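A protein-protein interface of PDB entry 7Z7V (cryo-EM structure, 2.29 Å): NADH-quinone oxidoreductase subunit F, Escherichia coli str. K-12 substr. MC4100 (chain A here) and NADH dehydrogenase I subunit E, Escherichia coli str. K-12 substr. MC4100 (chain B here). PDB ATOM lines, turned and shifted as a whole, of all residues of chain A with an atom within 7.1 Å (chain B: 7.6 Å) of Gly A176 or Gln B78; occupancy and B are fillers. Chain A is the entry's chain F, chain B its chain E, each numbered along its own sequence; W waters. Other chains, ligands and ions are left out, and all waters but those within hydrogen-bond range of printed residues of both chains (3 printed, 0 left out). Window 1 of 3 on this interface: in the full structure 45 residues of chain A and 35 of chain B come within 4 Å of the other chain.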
ATOM      1  N   ASP A  92       8.348 -21.527  15.674  1.00  0.00           N
ATOM      2  CA  ASP A  92       8.874 -21.703  17.022  1.00  0.00           C
ATOM      3  C   ASP A  92       8.741 -20.416  17.827  1.00  0.00           C
ATOM      4  O   ASP A  92       8.012 -20.376  18.820  1.00  0.00           O
ATOM      5  CB  ASP A  92      10.327 -22.170  16.968  1.00  0.00           C
ATOM      6  CG  ASP A  92      10.678 -23.111  18.104  1.00  0.00           C
ATOM      7  OD1 ASP A  92       9.942 -24.097  18.309  1.00  0.00           O
ATOM      8  OD2 ASP A  92      11.683 -22.862  18.800  1.00  0.00           O
ATOM      9  N   MET A  94      10.804 -18.334  19.822  1.00  0.00           N
ATOM     10  CA  MET A  94      11.188 -18.430  21.219  1.00  0.00           C
ATOM     11  C   MET A  94      12.105 -17.303  21.663  1.00  0.00           C
ATOM     12  O   MET A  94      12.543 -17.305  22.816  1.00  0.00           O
ATOM     13  CB  MET A  94      11.854 -19.783  21.482  1.00  0.00           C
ATOM     14  CG  MET A  94      10.892 -20.914  21.768  1.00  0.00           C
ATOM     15  SD  MET A  94      10.921 -21.407  23.491  1.00  0.00           S
ATOM     16  CE  MET A  94       9.771 -22.772  23.459  1.00  0.00           C
ATOM     17  N   ARG A 133       5.602 -24.010  18.366  1.00  0.00           N
ATOM     18  CA  ARG A 133       5.965 -24.199  19.763  1.00  0.00           C
ATOM     19  C   ARG A 133       4.764 -24.688  20.568  1.00  0.00           C
ATOM     20  O   ARG A 133       3.607 -24.425  20.230  1.00  0.00           O
ATOM     21  CB  ARG A 133       6.523 -22.903  20.355  1.00  0.00           C
ATOM     22  CG  ARG A 133       5.476 -21.885  20.754  1.00  0.00           C
ATOM     23  CD  ARG A 133       6.086 -20.611  21.297  1.00  0.00           C
ATOM     24  NE  ARG A 133       6.616 -20.759  22.643  1.00  0.00           N
ATOM     25  CZ  ARG A 133       7.194 -19.780  23.324  1.00  0.00           C
ATOM     26  NH1 ARG A 133       7.347 -18.574  22.804  1.00  0.00           N
ATOM     27  NH2 ARG A 133       7.624 -20.016  24.558  1.00  0.00           N
ATOM     28  N   GLY A 134       5.053 -25.436  21.634  1.00  0.00           N
ATOM     29  CA  GLY A 134       4.002 -26.083  22.398  1.00  0.00           C
ATOM     30  C   GLY A 134       3.177 -25.141  23.245  1.00  0.00           C
ATOM     31  O   GLY A 134       2.088 -25.517  23.687  1.00  0.00           O
ATOM     32  N   GLU A 135       3.668 -23.931  23.477  1.00  0.00           N
ATOM     33  CA  GLU A 135       2.999 -22.964  24.333  1.00  0.00           C
ATOM     34  C   GLU A 135       1.948 -22.153  23.593  1.00  0.00           C
ATOM     35  O   GLU A 135       1.178 -21.433  24.236  1.00  0.00           O
ATOM     36  CB  GLU A 135       4.033 -22.021  24.957  1.00  0.00           C
ATOM     37  CG  GLU A 135       5.025 -22.711  25.883  1.00  0.00           C
ATOM     38  CD  GLU A 135       6.185 -23.350  25.132  1.00  0.00           C
ATOM     39  OE1 GLU A 135       6.495 -22.890  24.015  1.00  0.00           O
ATOM     40  OE2 GLU A 135       6.772 -24.320  25.650  1.00  0.00           O
ATOM     41  N   THR A 173       3.668 -29.954  17.057  1.00  0.00           N
ATOM     42  CA  THR A 173       3.714 -29.158  18.275  1.00  0.00           C
ATOM     43  C   THR A 173       4.990 -29.458  19.052  1.00  0.00           C
ATOM     44  O   THR A 173       5.332 -30.624  19.272  1.00  0.00           O
ATOM     45  CB  THR A 173       2.485 -29.437  19.136  1.00  0.00           C
ATOM     46  OG1 THR A 173       1.334 -29.557  18.293  1.00  0.00           O
ATOM     47  CG2 THR A 173       2.254 -28.310  20.099  1.00  0.00           C
ATOM     48  N   GLY A 174       5.688 -28.402  19.469  1.00  0.00           N
ATOM     49  CA  GLY A 174       6.975 -28.556  20.111  1.00  0.00           C
ATOM     50  C   GLY A 174       6.885 -28.899  21.583  1.00  0.00           C
ATOM     51  O   GLY A 174       5.817 -28.938  22.188  1.00  0.00           O
ATOM     52  N   ALA A 175       8.055 -29.149  22.169  1.00  0.00           N
ATOM     53  CA  ALA A 175       8.157 -29.535  23.569  1.00  0.00           C
ATOM     54  C   ALA A 175       9.109 -28.623  24.334  1.00  0.00           C
ATOM     55  O   ALA A 175       9.744 -29.049  25.300  1.00  0.00           O
ATOM     56  CB  ALA A 175       8.584 -30.995  23.702  1.00  0.00           C
ATOM     57  N   GLY A 176       9.231 -27.373  23.902  1.00  0.00           N
ATOM     58  CA  GLY A 176       9.837 -26.342  24.719  1.00  0.00           C
ATOM     59  C   GLY A 176      11.347 -26.255  24.801  1.00  0.00           C
ATOM     60  O   GLY A 176      11.916 -26.441  25.878  1.00  0.00           O
ATOM     61  N   ARG A 177      12.009 -25.966  23.685  1.00  0.00           N
ATOM     62  CA  ARG A 177      13.406 -25.555  23.707  1.00  0.00           C
ATOM     63  C   ARG A 177      13.604 -24.446  22.687  1.00  0.00           C
ATOM     64  O   ARG A 177      13.054 -24.499  21.585  1.00  0.00           O
ATOM     65  CB  ARG A 177      14.358 -26.722  23.413  1.00  0.00           C
ATOM     66  CG  ARG A 177      14.707 -27.570  24.619  1.00  0.00           C
ATOM     67  CD  ARG A 177      15.439 -26.777  25.683  1.00  0.00           C
ATOM     68  NE  ARG A 177      15.844 -27.626  26.797  1.00  0.00           N
ATOM     69  CZ  ARG A 177      16.026 -27.204  28.039  1.00  0.00           C
ATOM     70  NH1 ARG A 177      15.859 -25.935  28.370  1.00  0.00           N
ATOM     71  NH2 ARG A 177      16.387 -28.078  28.974  1.00  0.00           N
ATOM     72  N   TYR A 178      14.392 -23.441  23.065  1.00  0.00           N
ATOM     73  CA  TYR A 178      14.607 -22.280  22.208  1.00  0.00           C
ATOM     74  C   TYR A 178      15.485 -22.614  21.010  1.00  0.00           C
ATOM     75  O   TYR A 178      15.341 -21.997  19.949  1.00  0.00           O
ATOM     76  CB  TYR A 178      15.209 -21.150  23.044  1.00  0.00           C
ATOM     77  CG  TYR A 178      15.944 -20.058  22.303  1.00  0.00           C
ATOM     78  CD1 TYR A 178      15.261 -18.996  21.733  1.00  0.00           C
ATOM     79  CD2 TYR A 178      17.326 -20.064  22.218  1.00  0.00           C
ATOM     80  CE1 TYR A 178      15.928 -17.988  21.079  1.00  0.00           C
ATOM     81  CE2 TYR A 178      17.996 -19.064  21.564  1.00  0.00           C
ATOM     82  CZ  TYR A 178      17.298 -18.031  20.999  1.00  0.00           C
ATOM     83  OH  TYR A 178      17.983 -17.036  20.352  1.00  0.00           O
ATOM     84  N   ILE A 179      16.383 -23.593  21.152  1.00  0.00           N
ATOM     85  CA  ILE A 179      17.266 -23.982  20.059  1.00  0.00           C
ATOM     86  C   ILE A 179      16.505 -24.657  18.921  1.00  0.00           C
ATOM     87  O   ILE A 179      17.004 -24.704  17.793  1.00  0.00           O
ATOM     88  CB  ILE A 179      18.400 -24.880  20.601  1.00  0.00           C
ATOM     89  CG1 ILE A 179      19.573 -24.971  19.615  1.00  0.00           C
ATOM     90  CG2 ILE A 179      17.882 -26.263  20.971  1.00  0.00           C
ATOM     91  CD1 ILE A 179      19.980 -23.661  19.005  1.00  0.00           C
ATOM     92  N   CYS A 180      15.285 -25.140  19.173  1.00  0.00           N
ATOM     93  CA  CYS A 180      14.487 -25.776  18.128  1.00  0.00           C
ATOM     94  C   CYS A 180      14.098 -24.817  17.015  1.00  0.00           C
ATOM     95  O   CYS A 180      13.715 -25.269  15.936  1.00  0.00           O
ATOM     96  CB  CYS A 180      13.218 -26.380  18.720  1.00  0.00           C
ATOM     97  SG  CYS A 180      13.510 -27.576  20.003  1.00  0.00           S
ATOM     98  N   GLU A 349      19.446 -22.287  27.672  1.00  0.00           N
ATOM     99  CA  GLU A 349      18.891 -22.714  26.398  1.00  0.00           C
ATOM    100  C   GLU A 349      19.960 -23.208  25.438  1.00  0.00           C
ATOM    101  O   GLU A 349      19.666 -23.441  24.264  1.00  0.00           O
ATOM    102  CB  GLU A 349      18.094 -21.581  25.756  1.00  0.00           C
ATOM    103  CG  GLU A 349      16.732 -21.373  26.385  1.00  0.00           C
ATOM    104  CD  GLU A 349      15.945 -22.660  26.521  1.00  0.00           C
ATOM    105  OE1 GLU A 349      15.692 -23.321  25.496  1.00  0.00           O
ATOM    106  OE2 GLU A 349      15.577 -23.013  27.658  1.00  0.00           O
ATOM    107  N   ILE B  37       8.612 -37.203  20.023  1.00  0.00           N
ATOM    108  CA  ILE B  37       8.220 -36.074  20.862  1.00  0.00           C
ATOM    109  C   ILE B  37       6.722 -36.104  21.126  1.00  0.00           C
ATOM    110  O   ILE B  37       6.273 -35.920  22.264  1.00  0.00           O
ATOM    111  CB  ILE B  37       8.658 -34.750  20.207  1.00  0.00           C
ATOM    112  CG1 ILE B  37      10.183 -34.639  20.198  1.00  0.00           C
ATOM    113  CG2 ILE B  37       8.050 -33.558  20.925  1.00  0.00           C
ATOM    114  CD1 ILE B  37      10.709 -33.559  19.285  1.00  0.00           C
ATOM    115  N   LEU B  40       5.827 -39.003  23.546  1.00  0.00           N
ATOM    116  CA  LEU B  40       6.095 -38.592  24.918  1.00  0.00           C
ATOM    117  C   LEU B  40       5.051 -37.597  25.407  1.00  0.00           C
ATOM    118  O   LEU B  40       4.616 -37.664  26.560  1.00  0.00           O
ATOM    119  CB  LEU B  40       7.496 -37.995  25.026  1.00  0.00           C
ATOM    120  CG  LEU B  40       8.661 -38.963  24.837  1.00  0.00           C
ATOM    121  CD1 LEU B  40       9.883 -38.211  24.366  1.00  0.00           C
ATOM    122  CD2 LEU B  40       8.953 -39.705  26.122  1.00  0.00           C
ATOM    123  N   LYS B  41       4.627 -36.678  24.537  1.00  0.00           N
ATOM    124  CA  LYS B  41       3.590 -35.722  24.908  1.00  0.00           C
ATOM    125  C   LYS B  41       2.240 -36.396  25.123  1.00  0.00           C
ATOM    126  O   LYS B  41       1.471 -35.959  25.978  1.00  0.00           O
ATOM    127  CB  LYS B  41       3.474 -34.633  23.843  1.00  0.00           C
ATOM    128  CG  LYS B  41       4.545 -33.567  23.944  1.00  0.00           C
ATOM    129  CD  LYS B  41       4.543 -32.661  22.730  1.00  0.00           C
ATOM    130  CE  LYS B  41       3.298 -31.800  22.684  1.00  0.00           C
ATOM    131  NZ  LYS B  41       3.627 -30.366  22.479  1.00  0.00           N
ATOM    132  N   GLN B  44       2.504 -38.056  28.492  1.00  0.00           N
ATOM    133  CA  GLN B  44       2.470 -37.007  29.505  1.00  0.00           C
ATOM    134  C   GLN B  44       1.073 -36.419  29.663  1.00  0.00           C
ATOM    135  O   GLN B  44       0.642 -36.128  30.780  1.00  0.00           O
ATOM    136  CB  GLN B  44       3.475 -35.912  29.149  1.00  0.00           C
ATOM    137  CG  GLN B  44       3.463 -34.728  30.088  1.00  0.00           C
ATOM    138  CD  GLN B  44       4.701 -33.881  29.969  1.00  0.00           C
ATOM    139  OE1 GLN B  44       5.799 -34.320  30.303  1.00  0.00           O
ATOM    140  NE2 GLN B  44       4.536 -32.654  29.496  1.00  0.00           N
ATOM    141  N   GLY B  48       0.166 -37.034  33.247  1.00  0.00           N
ATOM    142  CA  GLY B  48       0.803 -35.919  33.919  1.00  0.00           C
ATOM    143  C   GLY B  48       2.293 -35.799  33.664  1.00  0.00           C
ATOM    144  O   GLY B  48       2.818 -34.684  33.613  1.00  0.00           O
ATOM    145  N   TRP B  49       2.982 -36.923  33.499  1.00  0.00           N
ATOM    146  CA  TRP B  49       4.413 -36.950  33.247  1.00  0.00           C
ATOM    147  C   TRP B  49       4.730 -38.245  32.512  1.00  0.00           C
ATOM    148  O   TRP B  49       3.847 -39.065  32.254  1.00  0.00           O
ATOM    149  CB  TRP B  49       5.209 -36.823  34.552  1.00  0.00           C
ATOM    150  CG  TRP B  49       5.070 -37.999  35.474  1.00  0.00           C
ATOM    151  CD1 TRP B  49       3.924 -38.456  36.053  1.00  0.00           C
ATOM    152  CD2 TRP B  49       6.119 -38.856  35.932  1.00  0.00           C
ATOM    153  NE1 TRP B  49       4.192 -39.548  36.835  1.00  0.00           N
ATOM    154  CE2 TRP B  49       5.534 -39.815  36.780  1.00  0.00           C
ATOM    155  CE3 TRP B  49       7.496 -38.910  35.705  1.00  0.00           C
ATOM    156  CZ2 TRP B  49       6.275 -40.813  37.400  1.00  0.00           C
ATOM    157  CZ3 TRP B  49       8.230 -39.898  36.322  1.00  0.00           C
ATOM    158  CH2 TRP B  49       7.621 -40.837  37.161  1.00  0.00           C
ATOM    159  N   VAL B  50       6.000 -38.428  32.172  1.00  0.00           N
ATOM    160  CA  VAL B  50       6.453 -39.620  31.468  1.00  0.00           C
ATOM    161  C   VAL B  50       7.215 -40.487  32.468  1.00  0.00           C
ATOM    162  O   VAL B  50       8.351 -40.155  32.832  1.00  0.00           O
ATOM    163  CB  VAL B  50       7.327 -39.269  30.257  1.00  0.00           C
ATOM    164  CG1 VAL B  50       7.777 -40.530  29.553  1.00  0.00           C
ATOM    165  CG2 VAL B  50       6.576 -38.362  29.303  1.00  0.00           C
ATOM    166  N   ALA B  73      13.509 -37.201  25.690  1.00  0.00           N
ATOM    167  CA  ALA B  73      12.686 -36.804  26.831  1.00  0.00           C
ATOM    168  C   ALA B  73      13.448 -35.900  27.792  1.00  0.00           C
ATOM    169  O   ALA B  73      12.880 -34.947  28.336  1.00  0.00           O
ATOM    170  CB  ALA B  73      12.170 -38.043  27.560  1.00  0.00           C
ATOM    171  N   PHE B  75      16.053 -34.042  26.829  1.00  0.00           N
ATOM    172  CA  PHE B  75      16.452 -32.819  26.141  1.00  0.00           C
ATOM    173  C   PHE B  75      15.393 -31.732  26.285  1.00  0.00           C
ATOM    174  O   PHE B  75      15.710 -30.584  26.611  1.00  0.00           O
ATOM    175  CB  PHE B  75      16.726 -33.101  24.663  1.00  0.00           C
ATOM    176  CG  PHE B  75      17.250 -31.912  23.907  1.00  0.00           C
ATOM    177  CD1 PHE B  75      18.596 -31.593  23.946  1.00  0.00           C
ATOM    178  CD2 PHE B  75      16.397 -31.108  23.167  1.00  0.00           C
ATOM    179  CE1 PHE B  75      19.082 -30.500  23.261  1.00  0.00           C
ATOM    180  CE2 PHE B  75      16.878 -30.012  22.484  1.00  0.00           C
ATOM    181  CZ  PHE B  75      18.221 -29.709  22.526  1.00  0.00           C
ATOM    182  N   TYR B  76      14.131 -32.072  26.046  1.00  0.00           N
ATOM    183  CA  TYR B  76      13.070 -31.080  25.958  1.00  0.00           C
ATOM    184  C   TYR B  76      12.506 -30.793  27.340  1.00  0.00           C
ATOM    185  O   TYR B  76      12.162 -31.714  28.084  1.00  0.00           O
ATOM    186  CB  TYR B  76      11.974 -31.550  25.002  1.00  0.00           C
ATOM    187  CG  TYR B  76      12.459 -31.660  23.579  1.00  0.00           C
ATOM    188  CD1 TYR B  76      12.534 -30.545  22.762  1.00  0.00           C
ATOM    189  CD2 TYR B  76      12.873 -32.874  23.062  1.00  0.00           C
ATOM    190  CE1 TYR B  76      12.990 -30.648  21.471  1.00  0.00           C
ATOM    191  CE2 TYR B  76      13.333 -32.984  21.779  1.00  0.00           C
ATOM    192  CZ  TYR B  76      13.389 -31.869  20.986  1.00  0.00           C
ATOM    193  OH  TYR B  76      13.849 -31.980  19.701  1.00  0.00           O
ATOM    194  N   SER B  77      12.416 -29.505  27.676  1.00  0.00           N
ATOM    195  CA  SER B  77      12.095 -29.109  29.042  1.00  0.00           C
ATOM    196  C   SER B  77      10.634 -29.361  29.388  1.00  0.00           C
ATOM    197  O   SER B  77      10.309 -29.565  30.561  1.00  0.00           O
ATOM    198  CB  SER B  77      12.442 -27.638  29.254  1.00  0.00           C
ATOM    199  OG  SER B  77      12.013 -26.848  28.164  1.00  0.00           O
ATOM    200  N   GLN B  78       9.746 -29.356  28.403  1.00  0.00           N
ATOM    201  CA  GLN B  78       8.325 -29.527  28.668  1.00  0.00           C
ATOM    202  C   GLN B  78       7.892 -30.984  28.702  1.00  0.00           C
ATOM    203  O   GLN B  78       6.718 -31.258  28.962  1.00  0.00           O
ATOM    204  CB  GLN B  78       7.498 -28.760  27.636  1.00  0.00           C
ATOM    205  CG  GLN B  78       7.695 -27.258  27.697  1.00  0.00           C
ATOM    206  CD  GLN B  78       7.788 -26.736  29.120  1.00  0.00           C
ATOM    207  OE1 GLN B  78       6.869 -26.909  29.917  1.00  0.00           O
ATOM    208  NE2 GLN B  78       8.899 -26.089  29.440  1.00  0.00           N
ATOM    209  N   ILE B  79       8.799 -31.919  28.445  1.00  0.00           N
ATOM    210  CA  ILE B  79       8.540 -33.332  28.681  1.00  0.00           C
ATOM    211  C   ILE B  79       9.058 -33.646  30.078  1.00  0.00           C
ATOM    212  O   ILE B  79      10.262 -33.583  30.334  1.00  0.00           O
ATOM    213  CB  ILE B  79       9.200 -34.216  27.619  1.00  0.00           C
ATOM    214  CG1 ILE B  79       8.544 -33.976  26.259  1.00  0.00           C
ATOM    215  CG2 ILE B  79       9.104 -35.677  28.010  1.00  0.00           C
ATOM    216  CD1 ILE B  79       9.399 -34.378  25.093  1.00  0.00           C
ATOM    217  N   PHE B  80       8.145 -33.967  30.988  1.00  0.00           N
ATOM    218  CA  PHE B  80       8.477 -34.115  32.397  1.00  0.00           C
ATOM    219  C   PHE B  80       8.831 -35.566  32.694  1.00  0.00           C
ATOM    220  O   PHE B  80       8.011 -36.466  32.498  1.00  0.00           O
ATOM    221  CB  PHE B  80       7.318 -33.652  33.274  1.00  0.00           C
ATOM    222  CG  PHE B  80       6.938 -32.220  33.060  1.00  0.00           C
ATOM    223  CD1 PHE B  80       7.911 -31.246  32.935  1.00  0.00           C
ATOM    224  CD2 PHE B  80       5.610 -31.846  32.984  1.00  0.00           C
ATOM    225  CE1 PHE B  80       7.566 -29.926  32.739  1.00  0.00           C
ATOM    226  CE2 PHE B  80       5.260 -30.530  32.790  1.00  0.00           C
ATOM    227  CZ  PHE B  80       6.239 -29.569  32.664  1.00  0.00           C
ATOM    228  N   ARG B  81      10.055 -35.785  33.161  1.00  0.00           N
ATOM    229  CA  ARG B  81      10.522 -37.103  33.550  1.00  0.00           C
ATOM    230  C   ARG B  81      10.529 -37.290  35.060  1.00  0.00           C
ATOM    231  O   ARG B  81      11.059 -38.288  35.553  1.00  0.00           O
ATOM    232  CB  ARG B  81      11.911 -37.350  32.970  1.00  0.00           C
ATOM    233  CG  ARG B  81      11.896 -37.629  31.482  1.00  0.00           C
ATOM    234  CD  ARG B  81      11.251 -38.965  31.194  1.00  0.00           C
ATOM    235  NE  ARG B  81      12.152 -40.065  31.513  1.00  0.00           N
ATOM    236  CZ  ARG B  81      12.003 -40.885  32.543  1.00  0.00           C
ATOM    237  NH1 ARG B  81      10.978 -40.778  33.369  1.00  0.00           N
ATOM    238  NH2 ARG B  81      12.907 -41.837  32.747  1.00  0.00           N
ATOM    239  N   VAL B  88       0.433 -27.310  36.465  1.00  0.00           N
ATOM    240  CA  VAL B  88       1.786 -26.809  36.268  1.00  0.00           C
ATOM    241  C   VAL B  88       1.692 -25.316  35.996  1.00  0.00           C
ATOM    242  O   VAL B  88       1.164 -24.896  34.963  1.00  0.00           O
ATOM    243  CB  VAL B  88       2.500 -27.538  35.123  1.00  0.00           C
ATOM    244  CG1 VAL B  88       3.968 -27.155  35.088  1.00  0.00           C
ATOM    245  CG2 VAL B  88       2.335 -29.039  35.261  1.00  0.00           C
ATOM    246  N   ARG B  90       3.692 -22.109  34.955  1.00  0.00           N
ATOM    247  CA  ARG B  90       4.918 -21.761  34.245  1.00  0.00           C
ATOM    248  C   ARG B  90       4.964 -20.246  34.128  1.00  0.00           C
ATOM    249  O   ARG B  90       4.268 -19.663  33.295  1.00  0.00           O
ATOM    250  CB  ARG B  90       4.967 -22.421  32.875  1.00  0.00           C
ATOM    251  CG  ARG B  90       4.969 -23.927  32.913  1.00  0.00           C
ATOM    252  CD  ARG B  90       5.707 -24.479  31.703  1.00  0.00           C
ATOM    253  NE  ARG B  90       5.045 -24.323  30.405  1.00  0.00           N
ATOM    254  CZ  ARG B  90       3.792 -24.642  30.092  1.00  0.00           C
ATOM    255  NH1 ARG B  90       3.024 -25.360  30.898  1.00  0.00           N
ATOM    256  NH2 ARG B  90       3.314 -24.284  28.905  1.00  0.00           N
ATOM    257  N   LEU B 129       7.186 -23.595  38.024  1.00  0.00           N
ATOM    258  CA  LEU B 129       8.297 -23.707  37.109  1.00  0.00           C
ATOM    259  C   LEU B 129       8.546 -22.370  36.423  1.00  0.00           C
ATOM    260  O   LEU B 129       7.593 -21.739  35.923  1.00  0.00           O
ATOM    261  CB  LEU B 129       8.041 -24.792  36.060  1.00  0.00           C
ATOM    262  CG  LEU B 129       8.120 -26.255  36.495  1.00  0.00           C
ATOM    263  CD1 LEU B 129       7.731 -27.164  35.345  1.00  0.00           C
ATOM    264  CD2 LEU B 129       9.503 -26.595  37.010  1.00  0.00           C
ATOM    265  N   PRO B 130       9.790 -21.908  36.386  1.00  0.00           N
ATOM    266  CA  PRO B 130      10.141 -20.842  35.452  1.00  0.00           C
ATOM    267  C   PRO B 130      10.132 -21.378  34.034  1.00  0.00           C
ATOM    268  O   PRO B 130      10.348 -22.566  33.790  1.00  0.00           O
ATOM    269  CB  PRO B 130      11.551 -20.439  35.887  1.00  0.00           C
ATOM    270  CG  PRO B 130      12.109 -21.673  36.500  1.00  0.00           C
ATOM    271  CD  PRO B 130      10.957 -22.390  37.144  1.00  0.00           C
ATOM    272  N   THR B 131       9.864 -20.487  33.091  1.00  0.00           N
ATOM    273  CA  THR B 131       9.903 -20.865  31.691  1.00  0.00           C
ATOM    274  C   THR B 131      10.409 -19.682  30.889  1.00  0.00           C
ATOM    275  O   THR B 131      10.339 -18.533  31.329  1.00  0.00           O
ATOM    276  CB  THR B 131       8.530 -21.324  31.179  1.00  0.00           C
ATOM    277  OG1 THR B 131       8.662 -21.829  29.846  1.00  0.00           O
ATOM    278  CG2 THR B 131       7.529 -20.176  31.185  1.00  0.00           C
ATOM    279  N   CYS B 132      10.900 -19.975  29.691  1.00  0.00           N
ATOM    280  CA  CYS B 132      11.378 -18.935  28.797  1.00  0.00           C
ATOM    281  C   CYS B 132      10.202 -18.105  28.288  1.00  0.00           C
ATOM    282  O   CYS B 132       9.046 -18.310  28.671  1.00  0.00           O
ATOM    283  CB  CYS B 132      12.163 -19.553  27.643  1.00  0.00           C
ATOM    284  SG  CYS B 132      11.446 -21.071  26.996  1.00  0.00           S
HETATM  285  O   HOH W   1      10.159 -23.845  26.831  1.00  0.00           O
HETATM  286  O   HOH W   2      14.247 -21.737  29.446  1.00  0.00           O
HETATM  287  O   HOH W   3      13.111 -24.422  27.414  1.00  0.00           O
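The side-chain sulfur (SD) of Met A94 sits close to the guanidinium group (NH2) of Arg A133 (3.7 Å). O of Arg A177 sits close to SG of Cys A180 (3.5 Å). The guanidinium group (NH1) of Arg A177 lies within salt-bridge range of the side-chain carboxylate (OE2) of Glu A349. The backbone carbonyl oxygen of Gln B78 sits at hydrogen-bond distance from the side-chain amide nitrogen of Gln B44, 2.6 Å away. The side-chain amide nitrogen (NE2) of Gln B78 is in hydrogen-bond range of the side-chain hydroxyl (OG) of Ser B77, at 3.4 Å. The guanidinium group (NE) of Arg B90 is in hydrogen-bond range of the side-chain amide oxygen (OE1) of Gln B78 (3.2 Å).
The side-chain sulfur (SD) of Met A94 is in hydrogen-bond range of the side-chain sulfur (SG) of Cys B132 (3.6 Å). The side-chain amino group (NZ) of Lys B41 lies within hydrogen-bond range of the backbone carbonyl oxygen (O) of Gly A174 (2.6 Å). The backbone carbonyl oxygen (O) of Ala A175 lies within hydrogen-bond range of the backbone NH (N) of Gln B78, at 3.1 Å. O of Phe B75 lies within hydrogen-bond range of NE of Arg A177 (3.0 Å). The backbone carbonyl oxygen (O) of Gly A176 lies close to the side-chain hydroxyl (OG) of Ser B77 (2.3 Å).
Gln B78 touches just these residues of chain A: Glu A135 (3.7 Å), Ala A175 (3.1 Å) and Gly A176 (3.8 Å). Of the printed residues of chain B, Ala A175 touches Ile B37 (3.8 Å), Tyr B76 (3.4 Å), Ser B77 (3.6 Å), Gln B78 (3.1 Å) and Ile B79 (3.7 Å). Of the printed residues of chain B, Cys A180 touches Tyr B76. Printed residues of chain A within 4 Å of Arg B90: Glu A135 (3.8 Å). Ala B73 touches none of the printed residues of chain A. The nearest residue of chain A that does not touch Gln B78 is Gly A174 (5.7 Å).
Water W2 lies within hydrogen-bond range of the side-chain carboxylate (OE2) of Glu A349 and the side-chain sulfur (SG) of Cys B132. Water W3 lies within hydrogen-bond range of OG of Ser B77, O of Gly A176, OE2 of Glu A349, NH1 of Arg A177 and SG of Cys B132. Water W1 lies within hydrogen-bond range of the side-chain sulfur (SG) of Cys B132 (3.1 Å) and the backbone carbonyl oxygen (O) of Gly A176 (3.3 Å).
Of the 21 printed residues of chain B, 9 touch a printed residue of chain A. Hydrophobic or aromatic side chains of chain B within 4 Å of the printed part of chain A: Ile B37, Phe B75, Tyr B76 and Ile B79. Along chain B the printed residues that touch a printed residue of chain A span positions 37 to 132. Hydrophobic or aromatic side chains of chain A within 4 Å of the printed part of chain B: Met A94, Ala A175 and Ile A179. Among the printed residues, 16 pairs touch across the chains. Among the printed residues, no Asp or Glu carboxylate lies within 4 Å of a Lys or Arg side-chain nitrogen of the other chain.
CG of Gln B78 touches OE2 of Glu A135 (3.7 Å). Arg B90 touches Glu A135. Lys B41 touches Thr A173. Ala A175 touches Ile B37. Ala A175 touches Tyr B76 (O to CB, 3.4 Å). N of Ser B77 touches O of Ala A175, 3.6 Å away. Ile B79 touches Ala A175. Gln B78 touches Gly A176 (CG to CA, 3.8 Å). Arg A177 touches Ser B77. Ile A179 touches Phe B75.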
